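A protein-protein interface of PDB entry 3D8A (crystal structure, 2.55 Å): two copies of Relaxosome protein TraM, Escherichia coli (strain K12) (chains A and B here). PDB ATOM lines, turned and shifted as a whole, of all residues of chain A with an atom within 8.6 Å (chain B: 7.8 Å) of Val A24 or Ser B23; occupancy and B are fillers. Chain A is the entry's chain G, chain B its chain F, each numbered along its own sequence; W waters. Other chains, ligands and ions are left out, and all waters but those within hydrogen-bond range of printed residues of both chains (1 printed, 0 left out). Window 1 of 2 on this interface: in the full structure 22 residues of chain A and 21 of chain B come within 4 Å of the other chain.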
ATOM      1  N   CYS A  16     -16.683   1.200   5.191  1.00  0.00           N
ATOM      2  CA  CYS A  16     -17.989   1.831   5.013  1.00  0.00           C
ATOM      3  C   CYS A  16     -18.299   2.162   3.554  1.00  0.00           C
ATOM      4  O   CYS A  16     -19.373   1.809   3.065  1.00  0.00           O
ATOM      5  CB  CYS A  16     -18.116   3.089   5.875  1.00  0.00           C
ATOM      6  SG  CYS A  16     -18.190   2.766   7.650  1.00  0.00           S
ATOM      7  N   VAL A  17     -17.372   2.820   2.857  1.00  0.00           N
ATOM      8  CA  VAL A  17     -17.663   3.296   1.500  1.00  0.00           C
ATOM      9  C   VAL A  17     -17.750   2.170   0.480  1.00  0.00           C
ATOM     10  O   VAL A  17     -18.582   2.219  -0.435  1.00  0.00           O
ATOM     11  CB  VAL A  17     -16.705   4.425   1.029  1.00  0.00           C
ATOM     12  CG1 VAL A  17     -16.902   5.662   1.888  1.00  0.00           C
ATOM     13  CG2 VAL A  17     -15.258   3.973   1.064  1.00  0.00           C
ATOM     14  N   VAL A  18     -16.908   1.151   0.648  1.00  0.00           N
ATOM     15  CA  VAL A  18     -16.968  -0.042  -0.204  1.00  0.00           C
ATOM     16  C   VAL A  18     -18.250  -0.824   0.076  1.00  0.00           C
ATOM     17  O   VAL A  18     -18.946  -1.215  -0.858  1.00  0.00           O
ATOM     18  CB  VAL A  18     -15.705  -0.931  -0.083  1.00  0.00           C
ATOM     19  CG1 VAL A  18     -15.833  -2.207  -0.918  1.00  0.00           C
ATOM     20  CG2 VAL A  18     -14.487  -0.153  -0.535  1.00  0.00           C
ATOM     21  N   LYS A  19     -18.577  -1.014   1.350  1.00  0.00           N
ATOM     22  CA  LYS A  19     -19.807  -1.729   1.724  1.00  0.00           C
ATOM     23  C   LYS A  19     -21.059  -1.000   1.219  1.00  0.00           C
ATOM     24  O   LYS A  19     -21.974  -1.633   0.687  1.00  0.00           O
ATOM     25  CB  LYS A  19     -19.874  -1.985   3.236  1.00  0.00           C
ATOM     26  CG  LYS A  19     -20.871  -3.069   3.645  1.00  0.00           C
ATOM     27  CD  LYS A  19     -20.788  -3.406   5.131  1.00  0.00           C
ATOM     28  CE  LYS A  19     -19.578  -4.279   5.431  1.00  0.00           C
ATOM     29  NZ  LYS A  19     -19.359  -4.481   6.887  1.00  0.00           N
ATOM     30  N   THR A  20     -21.069   0.327   1.350  1.00  0.00           N
ATOM     31  CA  THR A  20     -22.163   1.159   0.857  1.00  0.00           C
ATOM     32  C   THR A  20     -22.316   1.094  -0.664  1.00  0.00           C
ATOM     33  O   THR A  20     -23.426   0.934  -1.159  1.00  0.00           O
ATOM     34  CB  THR A  20     -22.001   2.615   1.343  1.00  0.00           C
ATOM     35  OG1 THR A  20     -22.230   2.664   2.759  1.00  0.00           O
ATOM     36  CG2 THR A  20     -22.956   3.562   0.645  1.00  0.00           C
ATOM     37  N   GLN A  21     -21.214   1.193  -1.403  1.00  0.00           N
ATOM     38  CA  GLN A  21     -21.293   1.112  -2.863  1.00  0.00           C
ATOM     39  C   GLN A  21     -21.846  -0.234  -3.318  1.00  0.00           C
ATOM     40  O   GLN A  21     -22.699  -0.307  -4.217  1.00  0.00           O
ATOM     41  CB  GLN A  21     -19.941   1.383  -3.535  1.00  0.00           C
ATOM     42  CG  GLN A  21     -20.001   1.303  -5.067  1.00  0.00           C
ATOM     43  CD  GLN A  21     -21.225   2.042  -5.643  1.00  0.00           C
ATOM     44  OE1 GLN A  21     -21.473   3.210  -5.318  1.00  0.00           O
ATOM     45  NE2 GLN A  21     -21.987   1.357  -6.501  1.00  0.00           N
ATOM     46  N   SER A  22     -21.365  -1.302  -2.695  1.00  0.00           N
ATOM     47  CA  SER A  22     -21.824  -2.629  -3.050  1.00  0.00           C
ATOM     48  C   SER A  22     -23.308  -2.803  -2.700  1.00  0.00           C
ATOM     49  O   SER A  22     -24.061  -3.366  -3.485  1.00  0.00           O
ATOM     50  CB  SER A  22     -20.952  -3.684  -2.380  1.00  0.00           C
ATOM     51  OG  SER A  22     -21.153  -4.952  -2.975  1.00  0.00           O
ATOM     52  N   SER A  23     -23.723  -2.276  -1.549  1.00  0.00           N
ATOM     53  CA  SER A  23     -25.110  -2.379  -1.110  1.00  0.00           C
ATOM     54  C   SER A  23     -26.032  -1.549  -1.990  1.00  0.00           C
ATOM     55  O   SER A  23     -27.139  -1.974  -2.327  1.00  0.00           O
ATOM     56  CB  SER A  23     -25.242  -1.958   0.348  1.00  0.00           C
ATOM     57  OG  SER A  23     -24.321  -2.656   1.168  1.00  0.00           O
ATOM     58  N   VAL A  24     -25.553  -0.376  -2.378  1.00  0.00           N
ATOM     59  CA  VAL A  24     -26.302   0.540  -3.228  1.00  0.00           C
ATOM     60  C   VAL A  24     -26.476  -0.034  -4.646  1.00  0.00           C
ATOM     61  O   VAL A  24     -27.534   0.134  -5.269  1.00  0.00           O
ATOM     62  CB  VAL A  24     -25.628   1.939  -3.243  1.00  0.00           C
ATOM     63  CG1 VAL A  24     -26.041   2.752  -4.444  1.00  0.00           C
ATOM     64  CG2 VAL A  24     -25.949   2.692  -1.952  1.00  0.00           C
ATOM     65  N   ALA A  25     -25.454  -0.723  -5.151  1.00  0.00           N
ATOM     66  CA  ALA A  25     -25.571  -1.396  -6.455  1.00  0.00           C
ATOM     67  C   ALA A  25     -26.742  -2.381  -6.455  1.00  0.00           C
ATOM     68  O   ALA A  25     -27.526  -2.431  -7.406  1.00  0.00           O
ATOM     69  CB  ALA A  25     -24.282  -2.106  -6.837  1.00  0.00           C
ATOM     70  N   LYS A  26     -26.865  -3.141  -5.374  1.00  0.00           N
ATOM     71  CA  LYS A  26     -27.953  -4.099  -5.251  1.00  0.00           C
ATOM     72  C   LYS A  26     -29.317  -3.422  -5.130  1.00  0.00           C
ATOM     73  O   LYS A  26     -30.268  -3.836  -5.784  1.00  0.00           O
ATOM     74  CB  LYS A  26     -27.678  -5.098  -4.126  1.00  0.00           C
ATOM     75  CG  LYS A  26     -26.318  -5.781  -4.287  1.00  0.00           C
ATOM     76  CD  LYS A  26     -26.426  -7.292  -4.222  1.00  0.00           C
ATOM     77  CE  LYS A  26     -25.183  -7.985  -4.796  1.00  0.00           C
ATOM     78  NZ  LYS A  26     -23.923  -7.559  -4.127  1.00  0.00           N
ATOM     79  N   ILE A  27     -29.396  -2.363  -4.331  1.00  0.00           N
ATOM     80  CA  ILE A  27     -30.610  -1.573  -4.229  1.00  0.00           C
ATOM     81  C   ILE A  27     -31.011  -1.031  -5.594  1.00  0.00           C
ATOM     82  O   ILE A  27     -32.170  -1.129  -5.986  1.00  0.00           O
ATOM     83  CB  ILE A  27     -30.448  -0.417  -3.237  1.00  0.00           C
ATOM     84  CG1 ILE A  27     -30.251  -0.973  -1.822  1.00  0.00           C
ATOM     85  CG2 ILE A  27     -31.663   0.518  -3.303  1.00  0.00           C
ATOM     86  CD1 ILE A  27     -29.605  -0.006  -0.864  1.00  0.00           C
ATOM     87  N   LEU A  28     -30.050  -0.474  -6.322  1.00  0.00           N
ATOM     88  CA  LEU A  28     -30.294   0.012  -7.675  1.00  0.00           C
ATOM     89  C   LEU A  28     -30.870  -1.099  -8.553  1.00  0.00           C
ATOM     90  O   LEU A  28     -31.830  -0.882  -9.302  1.00  0.00           O
ATOM     91  CB  LEU A  28     -28.997   0.545  -8.292  1.00  0.00           C
ATOM     92  CG  LEU A  28     -29.047   1.274  -9.636  1.00  0.00           C
ATOM     93  CD1 LEU A  28     -29.831   2.578  -9.577  1.00  0.00           C
ATOM     94  CD2 LEU A  28     -27.631   1.543 -10.074  1.00  0.00           C
ATOM     95  N   GLY A  29     -30.283  -2.289  -8.449  1.00  0.00           N
ATOM     96  CA  GLY A  29     -30.762  -3.459  -9.181  1.00  0.00           C
ATOM     97  C   GLY A  29     -32.224  -3.763  -8.909  1.00  0.00           C
ATOM     98  O   GLY A  29     -33.019  -3.875  -9.834  1.00  0.00           O
ATOM     99  N   ILE A  30     -32.578  -3.881  -7.631  1.00  0.00           N
ATOM    100  CA  ILE A  30     -33.963  -4.145  -7.225  1.00  0.00           C
ATOM    101  C   ILE A  30     -34.907  -3.038  -7.702  1.00  0.00           C
ATOM    102  O   ILE A  30     -35.986  -3.323  -8.226  1.00  0.00           O
ATOM    103  CB  ILE A  30     -34.093  -4.360  -5.689  1.00  0.00           C
ATOM    104  CG1 ILE A  30     -33.393  -5.665  -5.277  1.00  0.00           C
ATOM    105  CG2 ILE A  30     -35.564  -4.330  -5.247  1.00  0.00           C
ATOM    106  CD1 ILE A  30     -33.605  -6.100  -3.820  1.00  0.00           C
ATOM    107  N   GLU A  31     -34.489  -1.785  -7.529  1.00  0.00           N
ATOM    108  CA  GLU A  31     -35.303  -0.638  -7.926  1.00  0.00           C
ATOM    109  C   GLU A  31     -35.556  -0.566  -9.429  1.00  0.00           C
ATOM    110  O   GLU A  31     -36.641  -0.175  -9.854  1.00  0.00           O
ATOM    111  CB  GLU A  31     -34.678   0.675  -7.434  1.00  0.00           C
ATOM    112  CG  GLU A  31     -34.831   0.928  -5.932  1.00  0.00           C
ATOM    113  CD  GLU A  31     -36.285   1.010  -5.491  1.00  0.00           C
ATOM    114  OE1 GLU A  31     -36.903   2.081  -5.670  1.00  0.00           O
ATOM    115  OE2 GLU A  31     -36.819   0.005  -4.966  1.00  0.00           O
ATOM    116  N   TYR A  45     -31.595  -0.870 -15.887  1.00  0.00           N
ATOM    117  CA  TYR A  45     -30.338  -1.068 -15.153  1.00  0.00           C
ATOM    118  C   TYR A  45     -29.085  -0.715 -15.951  1.00  0.00           C
ATOM    119  O   TYR A  45     -28.257   0.077 -15.505  1.00  0.00           O
ATOM    120  CB  TYR A  45     -30.238  -2.512 -14.642  1.00  0.00           C
ATOM    121  CG  TYR A  45     -29.122  -2.745 -13.644  1.00  0.00           C
ATOM    122  CD1 TYR A  45     -29.217  -2.271 -12.333  1.00  0.00           C
ATOM    123  CD2 TYR A  45     -27.972  -3.439 -14.003  1.00  0.00           C
ATOM    124  CE1 TYR A  45     -28.186  -2.480 -11.406  1.00  0.00           C
ATOM    125  CE2 TYR A  45     -26.936  -3.654 -13.080  1.00  0.00           C
ATOM    126  CZ  TYR A  45     -27.050  -3.176 -11.786  1.00  0.00           C
ATOM    127  OH  TYR A  45     -26.032  -3.396 -10.881  1.00  0.00           O
ATOM    128  N   MET A  48     -28.704   3.031 -16.624  1.00  0.00           N
ATOM    129  CA  MET A  48     -28.327   3.772 -15.437  1.00  0.00           C
ATOM    130  C   MET A  48     -26.857   3.556 -15.103  1.00  0.00           C
ATOM    131  O   MET A  48     -26.148   4.503 -14.764  1.00  0.00           O
ATOM    132  CB  MET A  48     -29.217   3.388 -14.256  1.00  0.00           C
ATOM    133  CG  MET A  48     -30.672   3.755 -14.438  1.00  0.00           C
ATOM    134  SD  MET A  48     -31.598   3.596 -12.904  1.00  0.00           S
ATOM    135  CE  MET A  48     -31.657   1.822 -12.676  1.00  0.00           C
ATOM    136  N   VAL A  49     -26.399   2.314 -15.206  1.00  0.00           N
ATOM    137  CA  VAL A  49     -24.985   1.994 -14.983  1.00  0.00           C
ATOM    138  C   VAL A  49     -24.076   2.759 -15.943  1.00  0.00           C
ATOM    139  O   VAL A  49     -23.021   3.254 -15.538  1.00  0.00           O
ATOM    140  CB  VAL A  49     -24.702   0.477 -15.125  1.00  0.00           C
ATOM    141  CG1 VAL A  49     -23.202   0.204 -15.167  1.00  0.00           C
ATOM    142  CG2 VAL A  49     -25.361  -0.290 -13.986  1.00  0.00           C
ATOM    143  N   ASP A  51     -24.728   5.680 -17.407  1.00  0.00           N
ATOM    144  CA  ASP A  51     -24.776   7.065 -16.923  1.00  0.00           C
ATOM    145  C   ASP A  51     -23.843   7.285 -15.731  1.00  0.00           C
ATOM    146  O   ASP A  51     -23.071   8.244 -15.702  1.00  0.00           O
ATOM    147  CB  ASP A  51     -26.210   7.421 -16.506  1.00  0.00           C
ATOM    148  CG  ASP A  51     -27.022   8.058 -17.626  1.00  0.00           C
ATOM    149  OD1 ASP A  51     -27.191   7.440 -18.707  1.00  0.00           O
ATOM    150  OD2 ASP A  51     -27.519   9.184 -17.404  1.00  0.00           O
ATOM    151  N   ILE A  52     -23.944   6.386 -14.753  1.00  0.00           N
ATOM    152  CA  ILE A  52     -23.161   6.450 -13.520  1.00  0.00           C
ATOM    153  C   ILE A  52     -21.656   6.378 -13.820  1.00  0.00           C
ATOM    154  O   ILE A  52     -20.881   7.188 -13.299  1.00  0.00           O
ATOM    155  CB  ILE A  52     -23.582   5.328 -12.533  1.00  0.00           C
ATOM    156  CG1 ILE A  52     -24.970   5.606 -11.975  1.00  0.00           C
ATOM    157  CG2 ILE A  52     -22.585   5.174 -11.394  1.00  0.00           C
ATOM    158  CD1 ILE A  52     -25.671   4.367 -11.485  1.00  0.00           C
ATOM    159  N   ARG A  53     -21.255   5.425 -14.664  1.00  0.00           N
ATOM    160  CA  ARG A  53     -19.842   5.259 -15.020  1.00  0.00           C
ATOM    161  C   ARG A  53     -19.276   6.492 -15.705  1.00  0.00           C
ATOM    162  O   ARG A  53     -18.137   6.882 -15.443  1.00  0.00           O
ATOM    163  CB  ARG A  53     -19.620   4.025 -15.890  1.00  0.00           C
ATOM    164  CG  ARG A  53     -19.383   2.776 -15.083  1.00  0.00           C
ATOM    165  CD  ARG A  53     -19.650   1.552 -15.915  1.00  0.00           C
ATOM    166  NE  ARG A  53     -19.107   0.351 -15.292  1.00  0.00           N
ATOM    167  CZ  ARG A  53     -19.437  -0.888 -15.639  1.00  0.00           C
ATOM    168  NH1 ARG A  53     -20.320  -1.095 -16.605  1.00  0.00           N
ATOM    169  NH2 ARG A  53     -18.889  -1.925 -15.016  1.00  0.00           N
ATOM    170  N   LYS A  55     -20.347   9.594 -15.214  1.00  0.00           N
ATOM    171  CA  LYS A  55     -20.182  10.598 -14.170  1.00  0.00           C
ATOM    172  C   LYS A  55     -18.908  10.357 -13.361  1.00  0.00           C
ATOM    173  O   LYS A  55     -18.173  11.304 -13.069  1.00  0.00           O
ATOM    174  CB  LYS A  55     -21.408  10.640 -13.249  1.00  0.00           C
ATOM    175  CG  LYS A  55     -21.307  11.615 -12.071  1.00  0.00           C
ATOM    176  CD  LYS A  55     -21.408  13.062 -12.518  1.00  0.00           C
ATOM    177  CE  LYS A  55     -21.365  14.014 -11.336  1.00  0.00           C
ATOM    178  NZ  LYS A  55     -21.585  15.413 -11.778  1.00  0.00           N
ATOM    179  N   VAL A  56     -18.653   9.094 -13.019  1.00  0.00           N
ATOM    180  CA  VAL A  56     -17.462   8.698 -12.267  1.00  0.00           C
ATOM    181  C   VAL A  56     -16.199   9.052 -13.036  1.00  0.00           C
ATOM    182  O   VAL A  56     -15.298   9.683 -12.488  1.00  0.00           O
ATOM    183  CB  VAL A  56     -17.481   7.184 -11.930  1.00  0.00           C
ATOM    184  CG1 VAL A  56     -16.114   6.695 -11.442  1.00  0.00           C
ATOM    185  CG2 VAL A  56     -18.560   6.887 -10.895  1.00  0.00           C
ATOM    186  N   CYS B  16     -15.598   5.288  -4.990  1.00  0.00           N
ATOM    187  CA  CYS B  16     -16.739   4.802  -4.232  1.00  0.00           C
ATOM    188  C   CYS B  16     -17.754   5.890  -3.941  1.00  0.00           C
ATOM    189  O   CYS B  16     -18.933   5.697  -4.163  1.00  0.00           O
ATOM    190  CB  CYS B  16     -16.280   4.155  -2.937  1.00  0.00           C
ATOM    191  SG  CYS B  16     -15.483   2.575  -3.208  1.00  0.00           S
ATOM    192  N   VAL B  17     -17.300   7.039  -3.456  1.00  0.00           N
ATOM    193  CA  VAL B  17     -18.258   8.056  -3.039  1.00  0.00           C
ATOM    194  C   VAL B  17     -18.954   8.747  -4.208  1.00  0.00           C
ATOM    195  O   VAL B  17     -20.151   9.050  -4.116  1.00  0.00           O
ATOM    196  CB  VAL B  17     -17.666   9.058  -2.024  1.00  0.00           C
ATOM    197  CG1 VAL B  17     -17.368   8.332  -0.707  1.00  0.00           C
ATOM    198  CG2 VAL B  17     -16.423   9.757  -2.583  1.00  0.00           C
ATOM    199  N   VAL B  18     -18.226   8.962  -5.309  1.00  0.00           N
ATOM    200  CA  VAL B  18     -18.836   9.478  -6.539  1.00  0.00           C
ATOM    201  C   VAL B  18     -19.836   8.461  -7.110  1.00  0.00           C
ATOM    202  O   VAL B  18     -20.947   8.822  -7.496  1.00  0.00           O
ATOM    203  CB  VAL B  18     -17.797   9.826  -7.620  1.00  0.00           C
ATOM    204  CG1 VAL B  18     -18.484  10.308  -8.893  1.00  0.00           C
ATOM    205  CG2 VAL B  18     -16.824  10.889  -7.120  1.00  0.00           C
ATOM    206  N   LYS B  19     -19.437   7.190  -7.153  1.00  0.00           N
ATOM    207  CA  LYS B  19     -20.285   6.132  -7.683  1.00  0.00           C
ATOM    208  C   LYS B  19     -21.565   6.012  -6.859  1.00  0.00           C
ATOM    209  O   LYS B  19     -22.666   5.872  -7.413  1.00  0.00           O
ATOM    210  CB  LYS B  19     -19.545   4.809  -7.634  1.00  0.00           C
ATOM    211  CG  LYS B  19     -19.778   3.898  -8.805  1.00  0.00           C
ATOM    212  CD  LYS B  19     -18.915   2.665  -8.635  1.00  0.00           C
ATOM    213  CE  LYS B  19     -18.185   2.316  -9.916  1.00  0.00           C
ATOM    214  NZ  LYS B  19     -17.094   1.333  -9.655  1.00  0.00           N
ATOM    215  N   THR B  20     -21.408   6.061  -5.540  1.00  0.00           N
ATOM    216  CA  THR B  20     -22.520   5.967  -4.617  1.00  0.00           C
ATOM    217  C   THR B  20     -23.470   7.152  -4.782  1.00  0.00           C
ATOM    218  O   THR B  20     -24.670   6.946  -4.901  1.00  0.00           O
ATOM    219  CB  THR B  20     -22.032   5.815  -3.147  1.00  0.00           C
ATOM    220  OG1 THR B  20     -21.445   4.522  -2.965  1.00  0.00           O
ATOM    221  CG2 THR B  20     -23.170   5.945  -2.165  1.00  0.00           C
ATOM    222  N   GLN B  21     -22.936   8.377  -4.824  1.00  0.00           N
ATOM    223  CA  GLN B  21     -23.788   9.562  -5.000  1.00  0.00           C
ATOM    224  C   GLN B  21     -24.620   9.473  -6.280  1.00  0.00           C
ATOM    225  O   GLN B  21     -25.827   9.756  -6.286  1.00  0.00           O
ATOM    226  CB  GLN B  21     -22.979  10.863  -5.014  1.00  0.00           C
ATOM    227  CG  GLN B  21     -23.873  12.109  -5.152  1.00  0.00           C
ATOM    228  CD  GLN B  21     -25.173  11.982  -4.345  1.00  0.00           C
ATOM    229  OE1 GLN B  21     -25.146  11.713  -3.143  1.00  0.00           O
ATOM    230  NE2 GLN B  21     -26.314  12.155  -5.014  1.00  0.00           N
ATOM    231  N   SER B  22     -23.966   9.073  -7.357  1.00  0.00           N
ATOM    232  CA  SER B  22     -24.638   8.966  -8.629  1.00  0.00           C
ATOM    233  C   SER B  22     -25.715   7.864  -8.584  1.00  0.00           C
ATOM    234  O   SER B  22     -26.837   8.062  -9.070  1.00  0.00           O
ATOM    235  CB  SER B  22     -23.616   8.704  -9.729  1.00  0.00           C
ATOM    236  OG  SER B  22     -23.808   9.615 -10.786  1.00  0.00           O
ATOM    237  N   SER B  23     -25.375   6.726  -7.978  1.00  0.00           N
ATOM    238  CA  SER B  23     -26.301   5.603  -7.862  1.00  0.00           C
ATOM    239  C   SER B  23     -27.515   5.962  -7.013  1.00  0.00           C
ATOM    240  O   SER B  23     -28.658   5.607  -7.336  1.00  0.00           O
ATOM    241  CB  SER B  23     -25.595   4.401  -7.246  1.00  0.00           C
ATOM    242  OG  SER B  23     -24.427   4.069  -7.965  1.00  0.00           O
ATOM    243  N   VAL B  24     -27.242   6.681  -5.932  1.00  0.00           N
ATOM    244  CA  VAL B  24     -28.245   7.060  -4.969  1.00  0.00           C
ATOM    245  C   VAL B  24     -29.202   8.101  -5.568  1.00  0.00           C
ATOM    246  O   VAL B  24     -30.401   8.056  -5.292  1.00  0.00           O
ATOM    247  CB  VAL B  24     -27.549   7.486  -3.665  1.00  0.00           C
ATOM    248  CG1 VAL B  24     -28.435   8.338  -2.793  1.00  0.00           C
ATOM    249  CG2 VAL B  24     -27.072   6.246  -2.934  1.00  0.00           C
ATOM    250  N   ALA B  25     -28.682   8.986  -6.420  1.00  0.00           N
ATOM    251  CA  ALA B  25     -29.506   9.962  -7.135  1.00  0.00           C
ATOM    252  C   ALA B  25     -30.552   9.235  -7.996  1.00  0.00           C
ATOM    253  O   ALA B  25     -31.726   9.607  -8.022  1.00  0.00           O
ATOM    254  CB  ALA B  25     -28.630  10.887  -7.980  1.00  0.00           C
ATOM    255  N   LYS B  26     -30.131   8.171  -8.667  1.00  0.00           N
ATOM    256  CA  LYS B  26     -31.056   7.377  -9.471  1.00  0.00           C
ATOM    257  C   LYS B  26     -32.084   6.624  -8.627  1.00  0.00           C
ATOM    258  O   LYS B  26     -33.267   6.580  -8.994  1.00  0.00           O
ATOM    259  CB  LYS B  26     -30.319   6.450 -10.447  1.00  0.00           C
ATOM    260  CG  LYS B  26     -29.282   7.192 -11.292  1.00  0.00           C
ATOM    261  CD  LYS B  26     -29.136   6.626 -12.666  1.00  0.00           C
ATOM    262  CE  LYS B  26     -29.690   7.568 -13.726  1.00  0.00           C
ATOM    263  NZ  LYS B  26     -28.692   8.605 -14.128  1.00  0.00           N
ATOM    264  N   ILE B  27     -31.649   6.059  -7.498  1.00  0.00           N
ATOM    265  CA  ILE B  27     -32.565   5.403  -6.571  1.00  0.00           C
ATOM    266  C   ILE B  27     -33.591   6.423  -6.054  1.00  0.00           C
ATOM    267  O   ILE B  27     -34.793   6.148  -6.035  1.00  0.00           O
ATOM    268  CB  ILE B  27     -31.825   4.702  -5.395  1.00  0.00           C
ATOM    269  CG1 ILE B  27     -30.953   3.553  -5.918  1.00  0.00           C
ATOM    270  CG2 ILE B  27     -32.819   4.178  -4.360  1.00  0.00           C
ATOM    271  CD1 ILE B  27     -29.800   3.152  -4.997  1.00  0.00           C
ATOM    272  N   LEU B  28     -33.113   7.600  -5.668  1.00  0.00           N
ATOM    273  CA  LEU B  28     -33.986   8.687  -5.236  1.00  0.00           C
ATOM    274  C   LEU B  28     -35.062   8.979  -6.298  1.00  0.00           C
ATOM    275  O   LEU B  28     -36.257   9.072  -5.983  1.00  0.00           O
ATOM    276  CB  LEU B  28     -33.144   9.935  -4.949  1.00  0.00           C
ATOM    277  CG  LEU B  28     -33.716  11.080  -4.108  1.00  0.00           C
ATOM    278  CD1 LEU B  28     -34.149  10.618  -2.723  1.00  0.00           C
ATOM    279  CD2 LEU B  28     -32.694  12.188  -3.979  1.00  0.00           C
ATOM    280  N   GLY B  29     -34.622   9.095  -7.554  1.00  0.00           N
ATOM    281  CA  GLY B  29     -35.506   9.311  -8.692  1.00  0.00           C
ATOM    282  C   GLY B  29     -36.594   8.263  -8.778  1.00  0.00           C
ATOM    283  O   GLY B  29     -37.775   8.596  -8.799  1.00  0.00           O
ATOM    284  N   ILE B  30     -36.197   6.994  -8.794  1.00  0.00           N
ATOM    285  CA  ILE B  30     -37.152   5.895  -8.859  1.00  0.00           C
ATOM    286  C   ILE B  30     -38.122   5.922  -7.677  1.00  0.00           C
ATOM    287  O   ILE B  30     -39.339   5.770  -7.867  1.00  0.00           O
ATOM    288  CB  ILE B  30     -36.444   4.524  -8.962  1.00  0.00           C
ATOM    289  CG1 ILE B  30     -35.768   4.384 -10.329  1.00  0.00           C
ATOM    290  CG2 ILE B  30     -37.433   3.383  -8.721  1.00  0.00           C
ATOM    291  CD1 ILE B  30     -34.789   3.242 -10.422  1.00  0.00           C
HETATM  292  O   HOH W   1     -19.623   4.681  -1.233  1.00  0.00           O
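The side-chain hydroxyl (OG1) of Thr B20 is in hydrogen-bond range of the side-chain amide oxygen (OE1) of Gln A21, at 2.7 Å. The side-chain amino group of Lys B26 is in salt-bridge range of the side-chain carboxylate of Asp A51.
The side-chain hydroxyl (OG1) of Thr B20 is in hydrogen-bond range of the backbone carbonyl oxygen (O) of Cys B16 (3.0 Å). The side-chain hydroxyl (OG) of Ser B23 lies within hydrogen-bond range of the backbone carbonyl oxygen (O) of Lys B19 (2.6 Å). The backbone carbonyl oxygen (O) of Cys A16 lies within hydrogen-bond range of the side-chain hydroxyl (OG1) of Thr A20 (3.0 Å).
Among the printed residues, merely in contact across the chains: Val A17 with Cys B16 (3.9 Å), Val A17 with Val B17 (3.8 Å), Val A18 with Cys B16 (3.9 Å), Thr A20 with Thr B20 (3.7 Å), Gln A21 with Cys B16 (3.7 Å), Gln A21 with Lys B19 (3.2 Å), Gln A21 with Ser B23 (3.9 Å), Val A24 with Ser B23 (3.3 Å), Val A24 with Val B24 (3.9 Å), Val A24 with Ile B27 (3.8 Å), Ile A27 with Ile B27 (3.6 Å), Leu A28 with Ser B23 (3.9 Å), Leu A28 with Lys B26 (3.998 Å), Leu A28 with Ile B27 (3.9 Å), Glu A31 with Ile B30 (3.4 Å), Met A48 with Lys B26 (3.6 Å), Ile A52 with Ser B23 (3.7 Å), Lys A55 with Ser B22 (3.5 Å), Val A56 with Val B18 (3.9 Å) and Val A56 with Lys B19 (3.7 Å).
Of chain B, only Ser B23 (3.3 Å), Val B24 (3.9 Å) and Ile B27 (3.8 Å) come within 4 Å of Val A24. No residue of chain B comes within 4 Å of Ala A25. Of the printed residues of chain B, Glu A31 touches Ile B30 (3.4 Å). Of the printed residues of chain B, Met A48 touches Lys B26 (3.6 Å). Arg A53 touches none of the printed residues of chain B. Of the printed residues of chain B, Val A56 touches Val B18 and Lys B19. Of chain A, only Lys A55 (3.5 Å) comes within 4 Å of Ser B22. Ser B23 touches just these residues of chain A: Gln A21 (3.9 Å), Val A24 (3.3 Å), Leu A28 (3.9 Å) and Ile A52 (3.7 Å). The nearest residue of chain B that does not touch Val A24 is Thr B20 (4.3 Å).
Among the printed residues, 22 pairs touch across the chains.
Val A17 touches Cys B16, but with the chains exchanged Cys A16 does not touch Val B17 (7.6 Å). Val B17 touches its own counterpart, Val A17. Val A24 touches Ile B27, but with the chains exchanged Ile A27 does not touch Val B24 (7.1 Å). Ile B27 touches its own counterpart, Ile A27.
Water W1 lies within hydrogen-bond range of OG1 of Thr B20 (2.5 Å), O of Val A17 (2.8 Å) and O of Cys B16 (3.2 Å).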
